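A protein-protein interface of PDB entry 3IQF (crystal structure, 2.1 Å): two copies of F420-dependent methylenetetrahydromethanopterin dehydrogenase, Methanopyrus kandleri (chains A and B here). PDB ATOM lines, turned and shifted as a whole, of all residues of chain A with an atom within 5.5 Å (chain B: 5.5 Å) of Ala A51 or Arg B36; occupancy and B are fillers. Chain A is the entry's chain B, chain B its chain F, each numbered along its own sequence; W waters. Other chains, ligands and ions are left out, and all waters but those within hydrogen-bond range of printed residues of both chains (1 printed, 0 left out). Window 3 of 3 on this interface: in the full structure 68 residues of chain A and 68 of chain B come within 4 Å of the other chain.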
ATOM      1  N   GLY A  39     -15.186  -3.571  18.970  1.00  0.00           N
ATOM      2  CA  GLY A  39     -14.086  -4.164  18.276  1.00  0.00           C
ATOM      3  C   GLY A  39     -14.140  -4.079  16.774  1.00  0.00           C
ATOM      4  O   GLY A  39     -15.058  -3.552  16.193  1.00  0.00           O
ATOM      5  N   THR A  40     -13.134  -4.668  16.160  1.00  0.00           N
ATOM      6  CA  THR A  40     -12.958  -4.626  14.710  1.00  0.00           C
ATOM      7  C   THR A  40     -13.008  -6.074  14.165  1.00  0.00           C
ATOM      8  O   THR A  40     -12.404  -6.402  13.160  1.00  0.00           O
ATOM      9  CB  THR A  40     -11.656  -3.918  14.366  1.00  0.00           C
ATOM     10  OG1 THR A  40     -10.544  -4.531  15.027  1.00  0.00           O
ATOM     11  CG2 THR A  40     -11.706  -2.368  14.761  1.00  0.00           C
ATOM     12  N   PRO A  46      -2.350  -2.612  13.306  1.00  0.00           N
ATOM     13  CA  PRO A  46      -2.316  -1.381  14.096  1.00  0.00           C
ATOM     14  C   PRO A  46      -3.434  -0.386  13.828  1.00  0.00           C
ATOM     15  O   PRO A  46      -3.966   0.214  14.762  1.00  0.00           O
ATOM     16  CB  PRO A  46      -0.963  -0.785  13.734  1.00  0.00           C
ATOM     17  CG  PRO A  46      -0.114  -1.963  13.463  1.00  0.00           C
ATOM     18  CD  PRO A  46      -1.017  -2.919  12.762  1.00  0.00           C
ATOM     19  N   GLU A  47      -3.774  -0.201  12.551  1.00  0.00           N
ATOM     20  CA  GLU A  47      -4.802   0.765  12.173  1.00  0.00           C
ATOM     21  C   GLU A  47      -6.160   0.327  12.745  1.00  0.00           C
ATOM     22  O   GLU A  47      -6.851   1.135  13.342  1.00  0.00           O
ATOM     23  CB  GLU A  47      -4.864   0.917  10.654  1.00  0.00           C
ATOM     24  CG  GLU A  47      -3.583   1.449  10.066  1.00  0.00           C
ATOM     25  CD  GLU A  47      -2.494   0.388   9.763  1.00  0.00           C
ATOM     26  OE1 GLU A  47      -2.503  -0.761  10.323  1.00  0.00           O
ATOM     27  OE2 GLU A  47      -1.604   0.755   8.941  1.00  0.00           O
ATOM     28  N   CYS A  48      -6.504  -0.961  12.583  1.00  0.00           N
ATOM     29  CA  CYS A  48      -7.757  -1.510  13.139  1.00  0.00           C
ATOM     30  C   CYS A  48      -7.785  -1.444  14.641  1.00  0.00           C
ATOM     31  O   CYS A  48      -8.799  -1.042  15.220  1.00  0.00           O
ATOM     32  CB  CYS A  48      -7.988  -2.964  12.714  1.00  0.00           C
ATOM     33  SG  CYS A  48      -8.019  -3.112  10.935  1.00  0.00           S
ATOM     34  N   VAL A  49      -6.667  -1.806  15.271  1.00  0.00           N
ATOM     35  CA  VAL A  49      -6.596  -1.804  16.728  1.00  0.00           C
ATOM     36  C   VAL A  49      -6.757  -0.391  17.275  1.00  0.00           C
ATOM     37  O   VAL A  49      -7.483  -0.189  18.220  1.00  0.00           O
ATOM     38  CB  VAL A  49      -5.314  -2.486  17.277  1.00  0.00           C
ATOM     39  CG1 VAL A  49      -5.269  -2.369  18.808  1.00  0.00           C
ATOM     40  CG2 VAL A  49      -5.265  -3.991  16.877  1.00  0.00           C
ATOM     41  N   GLU A  50      -6.118   0.597  16.640  1.00  0.00           N
ATOM     42  CA  GLU A  50      -6.244   1.987  17.070  1.00  0.00           C
ATOM     43  C   GLU A  50      -7.692   2.446  16.957  1.00  0.00           C
ATOM     44  O   GLU A  50      -8.193   3.129  17.843  1.00  0.00           O
ATOM     45  CB  GLU A  50      -5.351   2.885  16.230  1.00  0.00           C
ATOM     46  CG  GLU A  50      -5.507   4.390  16.503  1.00  0.00           C
ATOM     47  CD  GLU A  50      -4.480   5.241  15.729  1.00  0.00           C
ATOM     48  OE1 GLU A  50      -4.552   6.464  15.829  1.00  0.00           O
ATOM     49  OE2 GLU A  50      -3.609   4.677  15.023  1.00  0.00           O
ATOM     50  N   ALA A  51      -8.349   2.075  15.850  1.00  0.00           N
ATOM     51  CA  ALA A  51      -9.761   2.399  15.658  1.00  0.00           C
ATOM     52  C   ALA A  51     -10.605   1.758  16.761  1.00  0.00           C
ATOM     53  O   ALA A  51     -11.525   2.379  17.284  1.00  0.00           O
ATOM     54  CB  ALA A  51     -10.251   1.949  14.289  1.00  0.00           C
ATOM     55  N   ALA A  52     -10.287   0.522  17.115  1.00  0.00           N
ATOM     56  CA  ALA A  52     -10.993  -0.159  18.204  1.00  0.00           C
ATOM     57  C   ALA A  52     -10.818   0.576  19.523  1.00  0.00           C
ATOM     58  O   ALA A  52     -11.771   0.825  20.236  1.00  0.00           O
ATOM     59  CB  ALA A  52     -10.493  -1.625  18.352  1.00  0.00           C
ATOM     60  N   VAL A  53      -9.571   0.882  19.874  1.00  0.00           N
ATOM     61  CA  VAL A  53      -9.305   1.536  21.158  1.00  0.00           C
ATOM     62  C   VAL A  53      -9.939   2.932  21.210  1.00  0.00           C
ATOM     63  O   VAL A  53     -10.434   3.369  22.251  1.00  0.00           O
ATOM     64  CB  VAL A  53      -7.804   1.631  21.446  1.00  0.00           C
ATOM     65  CG1 VAL A  53      -7.567   2.358  22.739  1.00  0.00           C
ATOM     66  CG2 VAL A  53      -7.194   0.243  21.494  1.00  0.00           C
ATOM     67  N   GLU A  54      -9.923   3.619  20.075  1.00  0.00           N
ATOM     68  CA  GLU A  54     -10.564   4.921  19.937  1.00  0.00           C
ATOM     69  C   GLU A  54     -12.078   4.878  20.167  1.00  0.00           C
ATOM     70  O   GLU A  54     -12.626   5.738  20.838  1.00  0.00           O
ATOM     71  CB  GLU A  54     -10.328   5.457  18.531  1.00  0.00           C
ATOM     72  CG  GLU A  54      -9.015   6.166  18.253  1.00  0.00           C
ATOM     73  CD  GLU A  54      -9.072   6.897  16.894  1.00  0.00           C
ATOM     74  OE1 GLU A  54      -9.781   7.941  16.814  1.00  0.00           O
ATOM     75  OE2 GLU A  54      -8.452   6.426  15.894  1.00  0.00           O
ATOM     76  N   MET A  55     -12.743   3.870  19.590  1.00  0.00           N
ATOM     77  CA  MET A  55     -14.170   3.607  19.875  1.00  0.00           C
ATOM     78  C   MET A  55     -14.405   3.469  21.366  1.00  0.00           C
ATOM     79  O   MET A  55     -15.320   4.059  21.904  1.00  0.00           O
ATOM     80  CB  MET A  55     -14.643   2.294  19.245  1.00  0.00           C
ATOM     81  CG  MET A  55     -15.202   2.398  17.841  1.00  0.00           C
ATOM     82  SD  MET A  55     -16.004   0.829  17.414  1.00  0.00           S
ATOM     83  CE  MET A  55     -14.628  -0.314  17.149  1.00  0.00           C
ATOM     84  N   ALA A  56     -13.561   2.661  22.002  1.00  0.00           N
ATOM     85  CA  ALA A  56     -13.646   2.404  23.429  1.00  0.00           C
ATOM     86  C   ALA A  56     -13.516   3.682  24.225  1.00  0.00           C
ATOM     87  O   ALA A  56     -14.330   3.942  25.082  1.00  0.00           O
ATOM     88  CB  ALA A  56     -12.574   1.403  23.845  1.00  0.00           C
ATOM     89  N   ALA B   6     -19.614  -2.932   7.365  1.00  0.00           N
ATOM     90  CA  ALA B   6     -20.775  -3.312   8.149  1.00  0.00           C
ATOM     91  C   ALA B   6     -20.500  -3.122   9.616  1.00  0.00           C
ATOM     92  O   ALA B   6     -19.353  -3.301  10.100  1.00  0.00           O
ATOM     93  CB  ALA B   6     -21.137  -4.794   7.881  1.00  0.00           C
ATOM     94  N   ILE B   7     -21.576  -2.815  10.336  1.00  0.00           N
ATOM     95  CA  ILE B   7     -21.566  -2.851  11.799  1.00  0.00           C
ATOM     96  C   ILE B   7     -22.385  -4.045  12.280  1.00  0.00           C
ATOM     97  O   ILE B   7     -23.511  -4.244  11.794  1.00  0.00           O
ATOM     98  CB  ILE B   7     -22.134  -1.574  12.384  1.00  0.00           C
ATOM     99  CG1 ILE B   7     -21.335  -0.414  11.819  1.00  0.00           C
ATOM    100  CG2 ILE B   7     -22.030  -1.611  13.918  1.00  0.00           C
ATOM    101  CD1 ILE B   7     -21.727   0.969  12.352  1.00  0.00           C
ATOM    102  N   PHE B   8     -21.818  -4.810  13.221  1.00  0.00           N
ATOM    103  CA  PHE B   8     -22.523  -5.897  13.890  1.00  0.00           C
ATOM    104  C   PHE B   8     -22.827  -5.445  15.292  1.00  0.00           C
ATOM    105  O   PHE B   8     -21.964  -4.873  15.932  1.00  0.00           O
ATOM    106  CB  PHE B   8     -21.667  -7.151  13.919  1.00  0.00           C
ATOM    107  CG  PHE B   8     -21.480  -7.760  12.582  1.00  0.00           C
ATOM    108  CD1 PHE B   8     -20.486  -7.278  11.711  1.00  0.00           C
ATOM    109  CD2 PHE B   8     -22.276  -8.808  12.165  1.00  0.00           C
ATOM    110  CE1 PHE B   8     -20.324  -7.858  10.446  1.00  0.00           C
ATOM    111  CE2 PHE B   8     -22.124  -9.361  10.883  1.00  0.00           C
ATOM    112  CZ  PHE B   8     -21.150  -8.907  10.042  1.00  0.00           C
ATOM    113  N   GLU B  34     -14.567  -4.323   5.846  1.00  0.00           N
ATOM    114  CA  GLU B  34     -14.153  -3.739   7.124  1.00  0.00           C
ATOM    115  C   GLU B  34     -15.367  -3.738   8.047  1.00  0.00           C
ATOM    116  O   GLU B  34     -16.448  -3.293   7.643  1.00  0.00           O
ATOM    117  CB  GLU B  34     -13.646  -2.304   6.900  1.00  0.00           C
ATOM    118  CG  GLU B  34     -12.699  -1.795   7.966  1.00  0.00           C
ATOM    119  CD  GLU B  34     -11.995  -0.458   7.595  1.00  0.00           C
ATOM    120  OE1 GLU B  34     -11.810   0.400   8.496  1.00  0.00           O
ATOM    121  OE2 GLU B  34     -11.617  -0.264   6.413  1.00  0.00           O
ATOM    122  N   PHE B  35     -15.211  -4.291   9.252  1.00  0.00           N
ATOM    123  CA  PHE B  35     -16.329  -4.399  10.185  1.00  0.00           C
ATOM    124  C   PHE B  35     -16.019  -3.655  11.480  1.00  0.00           C
ATOM    125  O   PHE B  35     -14.857  -3.524  11.884  1.00  0.00           O
ATOM    126  CB  PHE B  35     -16.659  -5.850  10.577  1.00  0.00           C
ATOM    127  CG  PHE B  35     -16.909  -6.785   9.415  1.00  0.00           C
ATOM    128  CD1 PHE B  35     -16.346  -8.055   9.421  1.00  0.00           C
ATOM    129  CD2 PHE B  35     -17.688  -6.411   8.342  1.00  0.00           C
ATOM    130  CE1 PHE B  35     -16.585  -8.936   8.369  1.00  0.00           C
ATOM    131  CE2 PHE B  35     -17.917  -7.256   7.288  1.00  0.00           C
ATOM    132  CZ  PHE B  35     -17.363  -8.521   7.277  1.00  0.00           C
ATOM    133  N   ARG B  36     -17.094  -3.207  12.117  1.00  0.00           N
ATOM    134  CA  ARG B  36     -17.106  -2.785  13.501  1.00  0.00           C
ATOM    135  C   ARG B  36     -18.128  -3.620  14.266  1.00  0.00           C
ATOM    136  O   ARG B  36     -19.182  -3.963  13.737  1.00  0.00           O
ATOM    137  CB  ARG B  36     -17.502  -1.324  13.570  1.00  0.00           C
ATOM    138  CG  ARG B  36     -16.542  -0.443  12.852  1.00  0.00           C
ATOM    139  CD  ARG B  36     -15.166  -0.380  13.569  1.00  0.00           C
ATOM    140  NE  ARG B  36     -14.220   0.493  12.851  1.00  0.00           N
ATOM    141  CZ  ARG B  36     -13.318   0.072  11.955  1.00  0.00           C
ATOM    142  NH1 ARG B  36     -12.520   0.958  11.380  1.00  0.00           N
ATOM    143  NH2 ARG B  36     -13.210  -1.214  11.602  1.00  0.00           N
ATOM    144  N   VAL B  37     -17.798  -3.960  15.505  1.00  0.00           N
ATOM    145  CA  VAL B  37     -18.659  -4.811  16.327  1.00  0.00           C
ATOM    146  C   VAL B  37     -18.872  -4.046  17.643  1.00  0.00           C
ATOM    147  O   VAL B  37     -17.909  -3.565  18.253  1.00  0.00           O
ATOM    148  CB  VAL B  37     -18.038  -6.223  16.513  1.00  0.00           C
ATOM    149  CG1 VAL B  37     -18.910  -7.107  17.386  1.00  0.00           C
ATOM    150  CG2 VAL B  37     -17.768  -6.888  15.160  1.00  0.00           C
ATOM    151  N   VAL B  38     -20.131  -3.861  18.022  1.00  0.00           N
ATOM    152  CA  VAL B  38     -20.453  -3.208  19.290  1.00  0.00           C
ATOM    153  C   VAL B  38     -21.555  -3.999  19.990  1.00  0.00           C
ATOM    154  O   VAL B  38     -22.292  -4.763  19.357  1.00  0.00           O
ATOM    155  CB  VAL B  38     -20.888  -1.750  19.153  1.00  0.00           C
ATOM    156  CG1 VAL B  38     -19.800  -0.927  18.463  1.00  0.00           C
ATOM    157  CG2 VAL B  38     -22.230  -1.610  18.402  1.00  0.00           C
ATOM    158  N   ILE B  59     -21.220   5.500  15.686  1.00  0.00           N
ATOM    159  CA  ILE B  59     -20.100   5.061  14.861  1.00  0.00           C
ATOM    160  C   ILE B  59     -20.425   5.159  13.345  1.00  0.00           C
ATOM    161  O   ILE B  59     -19.562   5.488  12.549  1.00  0.00           O
ATOM    162  CB  ILE B  59     -19.641   3.635  15.270  1.00  0.00           C
ATOM    163  CG1 ILE B  59     -18.701   3.707  16.476  1.00  0.00           C
ATOM    164  CG2 ILE B  59     -18.915   2.910  14.127  1.00  0.00           C
ATOM    165  CD1 ILE B  59     -19.379   4.007  17.833  1.00  0.00           C
ATOM    166  N   PHE B  63     -18.299   6.029  10.124  1.00  0.00           N
ATOM    167  CA  PHE B  63     -17.907   4.764   9.494  1.00  0.00           C
ATOM    168  C   PHE B  63     -18.633   4.538   8.149  1.00  0.00           C
ATOM    169  O   PHE B  63     -18.088   3.936   7.245  1.00  0.00           O
ATOM    170  CB  PHE B  63     -18.106   3.606  10.492  1.00  0.00           C
ATOM    171  CG  PHE B  63     -17.543   2.285  10.034  1.00  0.00           C
ATOM    172  CD1 PHE B  63     -16.196   2.163   9.692  1.00  0.00           C
ATOM    173  CD2 PHE B  63     -18.369   1.166   9.929  1.00  0.00           C
ATOM    174  CE1 PHE B  63     -15.648   0.950   9.269  1.00  0.00           C
ATOM    175  CE2 PHE B  63     -17.842  -0.094   9.504  1.00  0.00           C
ATOM    176  CZ  PHE B  63     -16.473  -0.201   9.179  1.00  0.00           C
HETATM  177  O   HOH W   1     -12.818  -5.718  10.281  1.00  0.00           O
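Among the printed residues, pairs that only touch across the chains: Gly A39 with Arg B36, Thr A40 with Phe B35, Thr A40 with Arg B36, Ala A51 with Arg B36, Met A55 with Arg B36 and Met A55 with Ile B59.
The backbone carbonyl oxygen (O) of Arg B36 lies within hydrogen-bond range of the backbone NH (N) of Phe B8, 2.8 Å away.
O of Ala B6 is in hydrogen-bond range of N of Arg B36.
The side-chain carboxylate (OE1) of Glu B34 lies within salt-bridge range of the guanidinium group (NH1) of Arg B36 (3.0 Å).
Water W1 lies within hydrogen-bond range of the backbone NH of Phe B35 (3.0 Å) and the backbone carbonyl oxygen of Thr A40 (3.0 Å).
Of chain B, only Arg B36 (3.8 Å) comes within 4 Å of Ala A51.
Printed residues of chain B within 4 Å of Met A55: Arg B36 (3.6 Å) and Ile B59 (3.98 Å).
Of the printed residues of chain B, Gly A39 touches Arg B36 and Val B37.
The nearest printed residue of chain B that does not touch Ala A51 is Glu B34 (6.2 Å).
The nearest printed residue of chain A that does not touch Arg B36 is Cys A48 (5.6 Å).
No position is printed for both chains.
Hydrophobic or aromatic side chains of chain A that line the printed part of chain B: Ala A51 and Met A55.
Of the 10 printed residues of chain B, 4 touch a printed residue of chain A.
Printed residues of chain B that touch a printed residue of chain A: Phe B35, Arg B36, Val B37 and Ile B59.
Hydrophobic or aromatic side chains of chain B that line the printed part of chain A: Ile B59.
Along chain B the printed residues that touch a printed residue of chain A span positions 35 to 59.
Among the printed residues, 7 pairs touch across the chains.
Among the printed residues, no Asp or Glu carboxylate lies within 4 Å of a Lys or Arg side-chain nitrogen of the other chain.
O of Val B37 lies within hydrogen-bond range of N of Gly A39, at 2.8 Å.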
